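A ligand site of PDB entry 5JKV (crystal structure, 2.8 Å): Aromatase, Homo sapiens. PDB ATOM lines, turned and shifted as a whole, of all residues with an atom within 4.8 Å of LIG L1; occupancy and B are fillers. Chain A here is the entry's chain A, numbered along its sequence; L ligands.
The side-chain sulfur of Cys 437 is bound to an iron atom (FE1) of LIG L1, 2.2 Å away. An oxygen (O3) of LIG L1 lies within salt-bridge range of the guanidinium group of Arg 145 (2.6 Å). The guanidinium group (NH1) of Arg 115 is in salt-bridge range of an oxygen (O1) of LIG L1. NE of Arg 435 is in salt-bridge range of O4 of LIG L1 (2.7 Å). The guanidinium group of Arg 375 lies within salt-bridge range of an oxygen (O2) of LIG L1, 2.8 Å away. The indole nitrogen of Trp 141 is in hydrogen-bond range of an oxygen (O3) of LIG L1. O2 of LG2 L2 is in hydrogen-bond range of NH1 of Arg 115, at 3.3 Å.
The side-chain sulfur of Met 107 lies close to an oxygen (O2) of LIG L1 (3.7 Å). Merely in contact with LIG L1: Val 373 (3.1 Å), Phe 430 (3.3 Å), Ile 132 (3.3 Å), Met 447 (3.6 Å), Ser 314 (3.6 Å), Ala 306 (3.6 Å), Gly 436 (3.6 Å), Met 364 (3.6 Å), Gly 431 (3.6 Å), Met 446 (3.6 Å), Ile 133 (3.7 Å), Val 370 (3.8 Å), Pro 429 (3.8 Å), Leu 152 (3.8 Å), Thr 310 (3.8 Å), Gly 439 (3.9 Å), Ala 438 (3.9 Å), Met 311 (3.9 Å) and Ala 443 (3.999 Å). Hydrophobic or aromatic side chains within 4 Å of LIG L1: Met 107, Ile 132, Ile 133, Trp 141, Leu 152, Ala 306, Met 311, Met 364, Val 370, Val 373, Phe 430, Ala 438, Ala 443, Met 446 and Met 447. Of the 32 residues printed, 26 come within 4 Å of LIG L1.
O of Phe 430 lies within hydrogen-bond range of N of Cys 437, at 3.0 Å. SG of Cys 437 sits close to N of Gly 439. O of Gly 436 is in hydrogen-bond range of NH2 of Arg 145, at 2.9 Å. The guanidinium group (NE) of Arg 115 lies within hydrogen-bond range of the backbone carbonyl oxygen (O) of Ile 133, at 2.9 Å. NH2 of Arg 375 sits at hydrogen-bond distance from O of Arg 435, 3.5 Å away. The backbone carbonyl oxygen (O) of Ile 132 is in hydrogen-bond range of the guanidinium group (NH2) of Arg 435 (2.7 Å). The side-chain hydroxyl of Ser 314 is in hydrogen-bond range of the backbone carbonyl oxygen of Thr 310, at 2.7 Å. The backbone carbonyl oxygen (O) of Ala 306 sits at hydrogen-bond distance from the side-chain hydroxyl (OG1) of Thr 310.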
ATOM      1  N   MET A 107     -33.222   8.519  -8.239  1.00  0.00           N
ATOM      2  CA  MET A 107     -33.579   8.705  -9.656  1.00  0.00           C
ATOM      3  C   MET A 107     -34.858   7.950 -10.043  1.00  0.00           C
ATOM      4  O   MET A 107     -35.569   8.366 -10.972  1.00  0.00           O
ATOM      5  CB  MET A 107     -32.415   8.357 -10.588  1.00  0.00           C
ATOM      6  CG  MET A 107     -31.089   8.989 -10.171  1.00  0.00           C
ATOM      7  SD  MET A 107     -29.836   9.241 -11.458  1.00  0.00           S
ATOM      8  CE  MET A 107     -29.554   7.593 -12.031  1.00  0.00           C
ATOM      9  N   ARG A 115     -34.126  19.844  -9.177  1.00  0.00           N
ATOM     10  CA  ARG A 115     -32.714  20.149  -8.902  1.00  0.00           C
ATOM     11  C   ARG A 115     -32.705  21.282  -7.873  1.00  0.00           C
ATOM     12  O   ARG A 115     -33.725  21.535  -7.210  1.00  0.00           O
ATOM     13  CB  ARG A 115     -31.966  20.552 -10.184  1.00  0.00           C
ATOM     14  CG  ARG A 115     -32.222  19.645 -11.371  1.00  0.00           C
ATOM     15  CD  ARG A 115     -31.059  19.614 -12.341  1.00  0.00           C
ATOM     16  NE  ARG A 115     -31.365  18.737 -13.462  1.00  0.00           N
ATOM     17  CZ  ARG A 115     -31.129  17.421 -13.500  1.00  0.00           C
ATOM     18  NH1 ARG A 115     -30.554  16.802 -12.470  1.00  0.00           N
ATOM     19  NH2 ARG A 115     -31.468  16.723 -14.568  1.00  0.00           N
ATOM     20  N   ILE A 132     -35.973  23.325 -18.945  1.00  0.00           N
ATOM     21  CA  ILE A 132     -36.130  22.104 -18.160  1.00  0.00           C
ATOM     22  C   ILE A 132     -34.913  21.780 -17.283  1.00  0.00           C
ATOM     23  O   ILE A 132     -35.091  21.266 -16.183  1.00  0.00           O
ATOM     24  CB  ILE A 132     -36.588  20.853 -18.941  1.00  0.00           C
ATOM     25  CG1 ILE A 132     -35.627  20.449 -20.066  1.00  0.00           C
ATOM     26  CG2 ILE A 132     -38.021  21.007 -19.439  1.00  0.00           C
ATOM     27  CD1 ILE A 132     -35.740  18.979 -20.386  1.00  0.00           C
ATOM     28  N   ILE A 133     -33.704  22.082 -17.778  1.00  0.00           N
ATOM     29  CA  ILE A 133     -32.454  21.639 -17.125  1.00  0.00           C
ATOM     30  C   ILE A 133     -32.451  21.957 -15.626  1.00  0.00           C
ATOM     31  O   ILE A 133     -32.349  21.049 -14.807  1.00  0.00           O
ATOM     32  CB  ILE A 133     -31.166  22.154 -17.825  1.00  0.00           C
ATOM     33  CG1 ILE A 133     -31.175  21.815 -19.320  1.00  0.00           C
ATOM     34  CG2 ILE A 133     -29.933  21.544 -17.186  1.00  0.00           C
ATOM     35  CD1 ILE A 133     -30.156  22.583 -20.141  1.00  0.00           C
ATOM     36  N   TRP A 141     -42.035  22.121 -15.021  1.00  0.00           N
ATOM     37  CA  TRP A 141     -41.101  21.134 -15.560  1.00  0.00           C
ATOM     38  C   TRP A 141     -41.837  19.959 -16.213  1.00  0.00           C
ATOM     39  O   TRP A 141     -41.477  19.547 -17.321  1.00  0.00           O
ATOM     40  CB  TRP A 141     -40.134  20.664 -14.470  1.00  0.00           C
ATOM     41  CG  TRP A 141     -39.369  19.422 -14.820  1.00  0.00           C
ATOM     42  CD1 TRP A 141     -38.233  19.337 -15.579  1.00  0.00           C
ATOM     43  CD2 TRP A 141     -39.692  18.090 -14.444  1.00  0.00           C
ATOM     44  NE1 TRP A 141     -37.835  18.036 -15.689  1.00  0.00           N
ATOM     45  CE2 TRP A 141     -38.712  17.238 -14.994  1.00  0.00           C
ATOM     46  CE3 TRP A 141     -40.730  17.512 -13.683  1.00  0.00           C
ATOM     47  CZ2 TRP A 141     -38.714  15.847 -14.820  1.00  0.00           C
ATOM     48  CZ3 TRP A 141     -40.741  16.130 -13.499  1.00  0.00           C
ATOM     49  CH2 TRP A 141     -39.740  15.312 -14.065  1.00  0.00           C
ATOM     50  N   ARG A 145     -41.110  19.252 -20.218  1.00  0.00           N
ATOM     51  CA  ARG A 145     -40.291  18.085 -20.558  1.00  0.00           C
ATOM     52  C   ARG A 145     -40.767  17.244 -21.787  1.00  0.00           C
ATOM     53  O   ARG A 145     -39.913  16.863 -22.603  1.00  0.00           O
ATOM     54  CB  ARG A 145     -40.034  17.202 -19.327  1.00  0.00           C
ATOM     55  CG  ARG A 145     -38.936  16.165 -19.525  1.00  0.00           C
ATOM     56  CD  ARG A 145     -38.668  15.388 -18.259  1.00  0.00           C
ATOM     57  NE  ARG A 145     -38.085  14.067 -18.527  1.00  0.00           N
ATOM     58  CZ  ARG A 145     -36.782  13.793 -18.548  1.00  0.00           C
ATOM     59  NH1 ARG A 145     -35.876  14.729 -18.313  1.00  0.00           N
ATOM     60  NH2 ARG A 145     -36.378  12.549 -18.798  1.00  0.00           N
ATOM     61  N   PHE A 148     -39.181  18.105 -25.159  1.00  0.00           N
ATOM     62  CA  PHE A 148     -37.802  17.631 -25.290  1.00  0.00           C
ATOM     63  C   PHE A 148     -37.780  16.143 -25.606  1.00  0.00           C
ATOM     64  O   PHE A 148     -37.059  15.724 -26.508  1.00  0.00           O
ATOM     65  CB  PHE A 148     -36.992  17.951 -24.019  1.00  0.00           C
ATOM     66  CG  PHE A 148     -36.574  19.390 -23.905  1.00  0.00           C
ATOM     67  CD1 PHE A 148     -37.437  20.350 -23.371  1.00  0.00           C
ATOM     68  CD2 PHE A 148     -35.305  19.797 -24.335  1.00  0.00           C
ATOM     69  CE1 PHE A 148     -37.044  21.687 -23.272  1.00  0.00           C
ATOM     70  CE2 PHE A 148     -34.905  21.126 -24.235  1.00  0.00           C
ATOM     71  CZ  PHE A 148     -35.781  22.072 -23.698  1.00  0.00           C
ATOM     72  N   LEU A 152     -36.233  14.188 -29.089  1.00  0.00           N
ATOM     73  CA  LEU A 152     -34.988  13.452 -28.846  1.00  0.00           C
ATOM     74  C   LEU A 152     -35.121  11.918 -28.974  1.00  0.00           C
ATOM     75  O   LEU A 152     -34.187  11.170 -28.661  1.00  0.00           O
ATOM     76  CB  LEU A 152     -34.379  13.850 -27.498  1.00  0.00           C
ATOM     77  CG  LEU A 152     -33.933  15.312 -27.337  1.00  0.00           C
ATOM     78  CD1 LEU A 152     -33.748  15.673 -25.874  1.00  0.00           C
ATOM     79  CD2 LEU A 152     -32.668  15.642 -28.119  1.00  0.00           C
ATOM     80  N   PHE A 203     -33.411  20.661 -34.769  1.00  0.00           N
ATOM     81  CA  PHE A 203     -34.397  21.203 -33.816  1.00  0.00           C
ATOM     82  C   PHE A 203     -34.974  22.580 -34.154  1.00  0.00           C
ATOM     83  O   PHE A 203     -36.066  22.912 -33.706  1.00  0.00           O
ATOM     84  CB  PHE A 203     -33.841  21.220 -32.379  1.00  0.00           C
ATOM     85  CG  PHE A 203     -33.294  19.888 -31.927  1.00  0.00           C
ATOM     86  CD1 PHE A 203     -34.118  18.770 -31.829  1.00  0.00           C
ATOM     87  CD2 PHE A 203     -31.947  19.768 -31.566  1.00  0.00           C
ATOM     88  CE1 PHE A 203     -33.617  17.549 -31.395  1.00  0.00           C
ATOM     89  CE2 PHE A 203     -31.425  18.554 -31.132  1.00  0.00           C
ATOM     90  CZ  PHE A 203     -32.263  17.447 -31.057  1.00  0.00           C
ATOM     91  N   MET A 303     -31.959  23.586 -25.721  1.00  0.00           N
ATOM     92  CA  MET A 303     -31.793  22.527 -26.720  1.00  0.00           C
ATOM     93  C   MET A 303     -30.546  22.752 -27.577  1.00  0.00           C
ATOM     94  O   MET A 303     -29.853  21.789 -27.910  1.00  0.00           O
ATOM     95  CB  MET A 303     -33.055  22.436 -27.584  1.00  0.00           C
ATOM     96  CG  MET A 303     -33.084  21.272 -28.578  1.00  0.00           C
ATOM     97  SD  MET A 303     -33.066  19.626 -27.837  1.00  0.00           S
ATOM     98  CE  MET A 303     -34.801  19.201 -27.903  1.00  0.00           C
ATOM     99  N   ALA A 306     -27.061  22.236 -25.311  1.00  0.00           N
ATOM    100  CA  ALA A 306     -26.863  20.949 -24.645  1.00  0.00           C
ATOM    101  C   ALA A 306     -25.727  20.108 -25.247  1.00  0.00           C
ATOM    102  O   ALA A 306     -24.798  19.730 -24.525  1.00  0.00           O
ATOM    103  CB  ALA A 306     -28.163  20.156 -24.581  1.00  0.00           C
ATOM    104  N   ALA A 307     -25.796  19.853 -26.554  1.00  0.00           N
ATOM    105  CA  ALA A 307     -24.768  19.075 -27.237  1.00  0.00           C
ATOM    106  C   ALA A 307     -23.387  19.775 -27.317  1.00  0.00           C
ATOM    107  O   ALA A 307     -22.387  19.168 -26.934  1.00  0.00           O
ATOM    108  CB  ALA A 307     -25.261  18.606 -28.604  1.00  0.00           C
ATOM    109  N   THR A 310     -21.796  19.350 -23.700  1.00  0.00           N
ATOM    110  CA  THR A 310     -21.462  18.043 -23.141  1.00  0.00           C
ATOM    111  C   THR A 310     -20.866  17.060 -24.139  1.00  0.00           C
ATOM    112  O   THR A 310     -19.865  16.414 -23.831  1.00  0.00           O
ATOM    113  CB  THR A 310     -22.668  17.395 -22.431  1.00  0.00           C
ATOM    114  OG1 THR A 310     -23.877  17.646 -23.175  1.00  0.00           O
ATOM    115  CG2 THR A 310     -22.821  17.969 -21.054  1.00  0.00           C
ATOM    116  N   MET A 311     -21.484  16.962 -25.312  1.00  0.00           N
ATOM    117  CA  MET A 311     -21.080  16.017 -26.357  1.00  0.00           C
ATOM    118  C   MET A 311     -19.658  16.270 -26.833  1.00  0.00           C
ATOM    119  O   MET A 311     -18.867  15.344 -26.948  1.00  0.00           O
ATOM    120  CB  MET A 311     -22.029  16.091 -27.548  1.00  0.00           C
ATOM    121  CG  MET A 311     -23.398  15.475 -27.299  1.00  0.00           C
ATOM    122  SD  MET A 311     -23.425  13.739 -27.739  1.00  0.00           S
ATOM    123  CE  MET A 311     -22.802  13.798 -29.414  1.00  0.00           C
ATOM    124  N   SER A 314     -17.055  15.408 -24.235  1.00  0.00           N
ATOM    125  CA  SER A 314     -17.084  13.933 -24.139  1.00  0.00           C
ATOM    126  C   SER A 314     -16.327  13.263 -25.276  1.00  0.00           C
ATOM    127  O   SER A 314     -15.516  12.370 -25.042  1.00  0.00           O
ATOM    128  CB  SER A 314     -18.526  13.422 -24.119  1.00  0.00           C
ATOM    129  OG  SER A 314     -19.214  13.927 -22.997  1.00  0.00           O
ATOM    130  N   MET A 364     -16.860   7.202 -20.820  1.00  0.00           N
ATOM    131  CA  MET A 364     -17.752   7.938 -19.927  1.00  0.00           C
ATOM    132  C   MET A 364     -17.614   7.494 -18.471  1.00  0.00           C
ATOM    133  O   MET A 364     -17.703   8.326 -17.568  1.00  0.00           O
ATOM    134  CB  MET A 364     -19.198   7.805 -20.380  1.00  0.00           C
ATOM    135  CG  MET A 364     -19.553   8.661 -21.578  1.00  0.00           C
ATOM    136  SD  MET A 364     -21.167   8.241 -22.241  1.00  0.00           S
ATOM    137  CE  MET A 364     -22.213   9.141 -21.131  1.00  0.00           C
ATOM    138  N   VAL A 370     -19.940  14.750 -17.179  1.00  0.00           N
ATOM    139  CA  VAL A 370     -21.022  14.939 -16.223  1.00  0.00           C
ATOM    140  C   VAL A 370     -20.866  13.884 -15.118  1.00  0.00           C
ATOM    141  O   VAL A 370     -21.458  12.798 -15.176  1.00  0.00           O
ATOM    142  CB  VAL A 370     -22.420  14.883 -16.880  1.00  0.00           C
ATOM    143  CG1 VAL A 370     -23.483  15.374 -15.920  1.00  0.00           C
ATOM    144  CG2 VAL A 370     -22.449  15.708 -18.162  1.00  0.00           C
ATOM    145  N   VAL A 373     -24.742  14.823 -10.419  1.00  0.00           N
ATOM    146  CA  VAL A 373     -26.144  15.135 -10.688  1.00  0.00           C
ATOM    147  C   VAL A 373     -26.746  15.837  -9.464  1.00  0.00           C
ATOM    148  O   VAL A 373     -26.641  15.334  -8.344  1.00  0.00           O
ATOM    149  CB  VAL A 373     -26.963  13.863 -11.032  1.00  0.00           C
ATOM    150  CG1 VAL A 373     -28.429  14.186 -11.263  1.00  0.00           C
ATOM    151  CG2 VAL A 373     -26.389  13.160 -12.256  1.00  0.00           C
ATOM    152  N   ARG A 375     -29.956  17.159  -7.361  1.00  0.00           N
ATOM    153  CA  ARG A 375     -31.378  16.900  -7.106  1.00  0.00           C
ATOM    154  C   ARG A 375     -31.887  17.567  -5.806  1.00  0.00           C
ATOM    155  O   ARG A 375     -31.097  18.097  -5.023  1.00  0.00           O
ATOM    156  CB  ARG A 375     -31.674  15.393  -7.077  1.00  0.00           C
ATOM    157  CG  ARG A 375     -31.331  14.599  -8.339  1.00  0.00           C
ATOM    158  CD  ARG A 375     -32.162  15.018  -9.552  1.00  0.00           C
ATOM    159  NE  ARG A 375     -32.111  14.042 -10.635  1.00  0.00           N
ATOM    160  CZ  ARG A 375     -33.010  13.078 -10.826  1.00  0.00           C
ATOM    161  NH1 ARG A 375     -34.047  12.956  -9.993  1.00  0.00           N
ATOM    162  NH2 ARG A 375     -32.885  12.238 -11.838  1.00  0.00           N
ATOM    163  N   ILE A 398     -21.755  10.534  -9.312  1.00  0.00           N
ATOM    164  CA  ILE A 398     -21.755   9.333 -10.179  1.00  0.00           C
ATOM    165  C   ILE A 398     -20.363   8.942 -10.697  1.00  0.00           C
ATOM    166  O   ILE A 398     -20.102   7.765 -10.949  1.00  0.00           O
ATOM    167  CB  ILE A 398     -22.815   9.384 -11.317  1.00  0.00           C
ATOM    168  CG1 ILE A 398     -22.644  10.621 -12.195  1.00  0.00           C
ATOM    169  CG2 ILE A 398     -24.222   9.315 -10.717  1.00  0.00           C
ATOM    170  CD1 ILE A 398     -23.255  10.511 -13.578  1.00  0.00           C
ATOM    171  N   PRO A 429     -24.394   6.754 -16.505  1.00  0.00           N
ATOM    172  CA  PRO A 429     -23.726   7.905 -17.094  1.00  0.00           C
ATOM    173  C   PRO A 429     -24.671   9.035 -17.527  1.00  0.00           C
ATOM    174  O   PRO A 429     -24.236  10.183 -17.682  1.00  0.00           O
ATOM    175  CB  PRO A 429     -23.028   7.292 -18.320  1.00  0.00           C
ATOM    176  CG  PRO A 429     -23.922   6.181 -18.720  1.00  0.00           C
ATOM    177  CD  PRO A 429     -24.402   5.595 -17.418  1.00  0.00           C
ATOM    178  N   PHE A 430     -25.948   8.696 -17.725  1.00  0.00           N
ATOM    179  CA  PHE A 430     -26.951   9.639 -18.201  1.00  0.00           C
ATOM    180  C   PHE A 430     -28.022   9.957 -17.153  1.00  0.00           C
ATOM    181  O   PHE A 430     -28.771  10.914 -17.306  1.00  0.00           O
ATOM    182  CB  PHE A 430     -27.647   9.078 -19.434  1.00  0.00           C
ATOM    183  CG  PHE A 430     -26.773   8.993 -20.650  1.00  0.00           C
ATOM    184  CD1 PHE A 430     -26.340   7.758 -21.124  1.00  0.00           C
ATOM    185  CD2 PHE A 430     -26.409  10.153 -21.363  1.00  0.00           C
ATOM    186  CE1 PHE A 430     -25.544   7.662 -22.258  1.00  0.00           C
ATOM    187  CE2 PHE A 430     -25.612  10.057 -22.497  1.00  0.00           C
ATOM    188  CZ  PHE A 430     -25.179   8.811 -22.950  1.00  0.00           C
ATOM    189  N   GLY A 431     -28.099   9.129 -16.105  1.00  0.00           N
ATOM    190  CA  GLY A 431     -29.254   9.154 -15.225  1.00  0.00           C
ATOM    191  C   GLY A 431     -30.390   8.352 -15.847  1.00  0.00           C
ATOM    192  O   GLY A 431     -30.358   8.031 -17.052  1.00  0.00           O
ATOM    193  N   PHE A 432     -31.379   7.998 -15.039  1.00  0.00           N
ATOM    194  CA  PHE A 432     -32.582   7.296 -15.514  1.00  0.00           C
ATOM    195  C   PHE A 432     -33.815   7.823 -14.753  1.00  0.00           C
ATOM    196  O   PHE A 432     -33.692   8.673 -13.862  1.00  0.00           O
ATOM    197  CB  PHE A 432     -32.418   5.769 -15.378  1.00  0.00           C
ATOM    198  CG  PHE A 432     -32.688   5.244 -14.003  1.00  0.00           C
ATOM    199  CD1 PHE A 432     -33.939   4.691 -13.692  1.00  0.00           C
ATOM    200  CD2 PHE A 432     -31.730   5.326 -12.998  1.00  0.00           C
ATOM    201  CE1 PHE A 432     -34.211   4.237 -12.410  1.00  0.00           C
ATOM    202  CE2 PHE A 432     -31.987   4.874 -11.716  1.00  0.00           C
ATOM    203  CZ  PHE A 432     -33.239   4.333 -11.417  1.00  0.00           C
ATOM    204  N   ARG A 435     -36.598  12.093 -14.398  1.00  0.00           N
ATOM    205  CA  ARG A 435     -35.739  13.248 -14.683  1.00  0.00           C
ATOM    206  C   ARG A 435     -34.320  12.863 -15.161  1.00  0.00           C
ATOM    207  O   ARG A 435     -33.366  13.622 -14.969  1.00  0.00           O
ATOM    208  CB  ARG A 435     -35.720  14.228 -13.489  1.00  0.00           C
ATOM    209  CG  ARG A 435     -35.214  15.610 -13.851  1.00  0.00           C
ATOM    210  CD  ARG A 435     -35.722  16.716 -12.953  1.00  0.00           C
ATOM    211  NE  ARG A 435     -35.326  18.009 -13.504  1.00  0.00           N
ATOM    212  CZ  ARG A 435     -35.814  19.198 -13.135  1.00  0.00           C
ATOM    213  NH1 ARG A 435     -36.738  19.290 -12.183  1.00  0.00           N
ATOM    214  NH2 ARG A 435     -35.370  20.285 -13.725  1.00  0.00           N
ATOM    215  N   GLY A 436     -34.187  11.707 -15.812  1.00  0.00           N
ATOM    216  CA  GLY A 436     -32.922  11.284 -16.417  1.00  0.00           C
ATOM    217  C   GLY A 436     -32.653  12.108 -17.666  1.00  0.00           C
ATOM    218  O   GLY A 436     -33.550  12.825 -18.136  1.00  0.00           O
ATOM    219  N   CYS A 437     -31.433  12.001 -18.208  1.00  0.00           N
ATOM    220  CA  CYS A 437     -31.043  12.773 -19.398  1.00  0.00           C
ATOM    221  C   CYS A 437     -32.091  12.623 -20.494  1.00  0.00           C
ATOM    222  O   CYS A 437     -32.419  11.513 -20.901  1.00  0.00           O
ATOM    223  CB  CYS A 437     -29.671  12.343 -19.931  1.00  0.00           C
ATOM    224  SG  CYS A 437     -29.067  13.307 -21.351  1.00  0.00           S
ATOM    225  N   ALA A 438     -32.632  13.758 -20.926  1.00  0.00           N
ATOM    226  CA  ALA A 438     -33.636  13.794 -21.990  1.00  0.00           C
ATOM    227  C   ALA A 438     -33.061  13.298 -23.306  1.00  0.00           C
ATOM    228  O   ALA A 438     -33.764  12.709 -24.120  1.00  0.00           O
ATOM    229  CB  ALA A 438     -34.200  15.199 -22.150  1.00  0.00           C
ATOM    230  N   GLY A 439     -31.766  13.533 -23.507  1.00  0.00           N
ATOM    231  CA  GLY A 439     -31.073  13.135 -24.726  1.00  0.00           C
ATOM    232  C   GLY A 439     -30.280  11.849 -24.624  1.00  0.00           C
ATOM    233  O   GLY A 439     -29.443  11.589 -25.489  1.00  0.00           O
ATOM    234  N   ALA A 443     -27.944  10.755 -27.730  1.00  0.00           N
ATOM    235  CA  ALA A 443     -26.545  11.019 -27.438  1.00  0.00           C
ATOM    236  C   ALA A 443     -25.648   9.861 -27.871  1.00  0.00           C
ATOM    237  O   ALA A 443     -24.571  10.097 -28.437  1.00  0.00           O
ATOM    238  CB  ALA A 443     -26.350  11.319 -25.955  1.00  0.00           C
ATOM    239  N   MET A 446     -25.565   9.890 -31.720  1.00  0.00           N
ATOM    240  CA  MET A 446     -24.712  10.997 -32.170  1.00  0.00           C
ATOM    241  C   MET A 446     -23.226  10.717 -31.986  1.00  0.00           C
ATOM    242  O   MET A 446     -22.425  10.955 -32.909  1.00  0.00           O
ATOM    243  CB  MET A 446     -25.082  12.268 -31.428  1.00  0.00           C
ATOM    244  CG  MET A 446     -26.311  12.974 -31.959  1.00  0.00           C
ATOM    245  SD  MET A 446     -26.536  14.605 -31.231  1.00  0.00           S
ATOM    246  CE  MET A 446     -27.600  14.157 -29.863  1.00  0.00           C
ATOM    247  N   MET A 447     -22.852  10.215 -30.813  1.00  0.00           N
ATOM    248  CA  MET A 447     -21.457   9.890 -30.491  1.00  0.00           C
ATOM    249  C   MET A 447     -20.894   8.801 -31.382  1.00  0.00           C
ATOM    250  O   MET A 447     -19.735   8.874 -31.771  1.00  0.00           O
ATOM    251  CB  MET A 447     -21.286   9.515 -29.016  1.00  0.00           C
ATOM    252  CG  MET A 447     -21.174  10.737 -28.121  1.00  0.00           C
ATOM    253  SD  MET A 447     -20.841  10.384 -26.395  1.00  0.00           S
ATOM    254  CE  MET A 447     -22.415   9.761 -25.833  1.00  0.00           C
HETATM  255  C1  LIG L   1     -29.707  15.948 -18.090  1.00  0.00           C
HETATM  256  C2  LIG L   1     -25.728  13.414 -19.101  1.00  0.00           C
HETATM  257  C3  LIG L   1     -26.209  14.644 -23.737  1.00  0.00           C
HETATM  258  C4  LIG L   1     -30.256  17.079 -22.802  1.00  0.00           C
HETATM  259  C5  LIG L   1     -28.622  15.125 -17.967  1.00  0.00           C
HETATM  260  C6  LIG L   1     -28.195  14.469 -16.739  1.00  0.00           C
HETATM  261  C7  LIG L   1     -27.099  13.754 -17.027  1.00  0.00           C
HETATM  262  C8  LIG L   1     -26.805  13.946 -18.431  1.00  0.00           C
HETATM  263  C9  LIG L   1     -26.290  12.878 -16.037  1.00  0.00           C
HETATM  264  C10 LIG L   1     -28.907  14.546 -15.369  1.00  0.00           C
HETATM  265  C11 LIG L   1     -30.037  13.512 -15.368  1.00  0.00           C
HETATM  266  C12 LIG L   1     -30.584  13.252 -13.985  1.00  0.00           C
HETATM  267  O1  LIG L   1     -30.840  14.237 -13.218  1.00  0.00           O
HETATM  268  O2  LIG L   1     -30.776  12.055 -13.639  1.00  0.00           O
HETATM  269  C13 LIG L   1     -25.456  13.625 -20.428  1.00  0.00           C
HETATM  270  C14 LIG L   1     -24.235  13.257 -21.132  1.00  0.00           C
HETATM  271  C15 LIG L   1     -24.384  13.599 -22.411  1.00  0.00           C
HETATM  272  C16 LIG L   1     -25.695  14.191 -22.551  1.00  0.00           C
HETATM  273  C17 LIG L   1     -23.000  12.591 -20.486  1.00  0.00           C
HETATM  274  C18 LIG L   1     -23.388  13.458 -23.597  1.00  0.00           C
HETATM  275  C19 LIG L   1     -22.435  12.532 -23.600  1.00  0.00           C
HETATM  276  C20 LIG L   1     -27.361  15.374 -23.897  1.00  0.00           C
HETATM  277  C21 LIG L   1     -27.883  15.851 -25.158  1.00  0.00           C
HETATM  278  C22 LIG L   1     -29.020  16.532 -24.896  1.00  0.00           C
HETATM  279  C23 LIG L   1     -29.219  16.490 -23.464  1.00  0.00           C
HETATM  280  C24 LIG L   1     -27.237  15.599 -26.532  1.00  0.00           C
HETATM  281  C25 LIG L   1     -29.966  17.230 -25.900  1.00  0.00           C
HETATM  282  C26 LIG L   1     -29.501  17.861 -26.996  1.00  0.00           C
HETATM  283  C27 LIG L   1     -30.455  17.054 -21.443  1.00  0.00           C
HETATM  284  C28 LIG L   1     -31.503  17.781 -20.763  1.00  0.00           C
HETATM  285  C29 LIG L   1     -31.340  17.442 -19.282  1.00  0.00           C
HETATM  286  C30 LIG L   1     -30.203  16.530 -19.236  1.00  0.00           C
HETATM  287  C31 LIG L   1     -32.562  18.712 -21.399  1.00  0.00           C
HETATM  288  C32 LIG L   1     -32.226  17.948 -18.121  1.00  0.00           C
HETATM  289  C33 LIG L   1     -33.321  16.895 -17.924  1.00  0.00           C
HETATM  290  C34 LIG L   1     -34.324  17.287 -16.868  1.00  0.00           C
HETATM  291  O3  LIG L   1     -35.539  16.977 -17.030  1.00  0.00           O
HETATM  292  O4  LIG L   1     -33.927  17.923 -15.841  1.00  0.00           O
HETATM  293  N1  LIG L   1     -27.762  14.766 -18.968  1.00  0.00           N
HETATM  294  N2  LIG L   1     -26.319  14.177 -21.328  1.00  0.00           N
HETATM  295  N3  LIG L   1     -28.202  15.758 -22.879  1.00  0.00           N
HETATM  296  N4  LIG L   1     -29.714  16.331 -20.517  1.00  0.00           N
HETATM  297 FE1  LIG L   1     -27.998  15.214 -20.931  1.00  0.00          FE
HETATM  298  C1  LG2 L   2     -27.366  19.723 -19.389  1.00  0.00           C
HETATM  299  C2  LG2 L   2     -26.143  19.216 -18.585  1.00  0.00           C
HETATM  300  C3  LG2 L   2     -27.707  18.647 -16.563  1.00  0.00           C
HETATM  301  C4  LG2 L   2     -27.952  18.703 -15.045  1.00  0.00           C
HETATM  302  C5  LG2 L   2     -26.696  18.286 -14.275  1.00  0.00           C
HETATM  303  C6  LG2 L   2     -25.569  19.236 -14.678  1.00  0.00           C
HETATM  304  C7  LG2 L   2     -24.500  19.129 -13.583  1.00  0.00           C
HETATM  305  C8  LG2 L   2     -25.342  19.067 -12.303  1.00  0.00           C
HETATM  306  C9  LG2 L   2     -26.684  18.551 -12.798  1.00  0.00           C
HETATM  307  C10 LG2 L   2     -26.426  16.781 -14.425  1.00  0.00           C
HETATM  308  C11 LG2 L   2     -25.909  17.743 -18.942  1.00  0.00           C
HETATM  309  C12 LG2 L   2     -27.092  20.106 -20.843  1.00  0.00           C
HETATM  310  C13 LG2 L   2     -25.946  21.096 -20.858  1.00  0.00           C
HETATM  311  C14 LG2 L   2     -24.788  20.875 -19.957  1.00  0.00           C
HETATM  312  C15 LG2 L   2     -24.879  20.034 -18.896  1.00  0.00           C
HETATM  313  C16 LG2 L   2     -23.653  19.943 -18.004  1.00  0.00           C
HETATM  314  C17 LG2 L   2     -24.064  20.135 -16.549  1.00  0.00           C
HETATM  315  C18 LG2 L   2     -25.183  19.161 -16.162  1.00  0.00           C
HETATM  316  C19 LG2 L   2     -26.440  19.394 -17.056  1.00  0.00           C
HETATM  317  O1  LG2 L   2     -25.994  22.061 -21.594  1.00  0.00           O
HETATM  318  O2  LG2 L   2     -27.649  18.358 -12.066  1.00  0.00           O
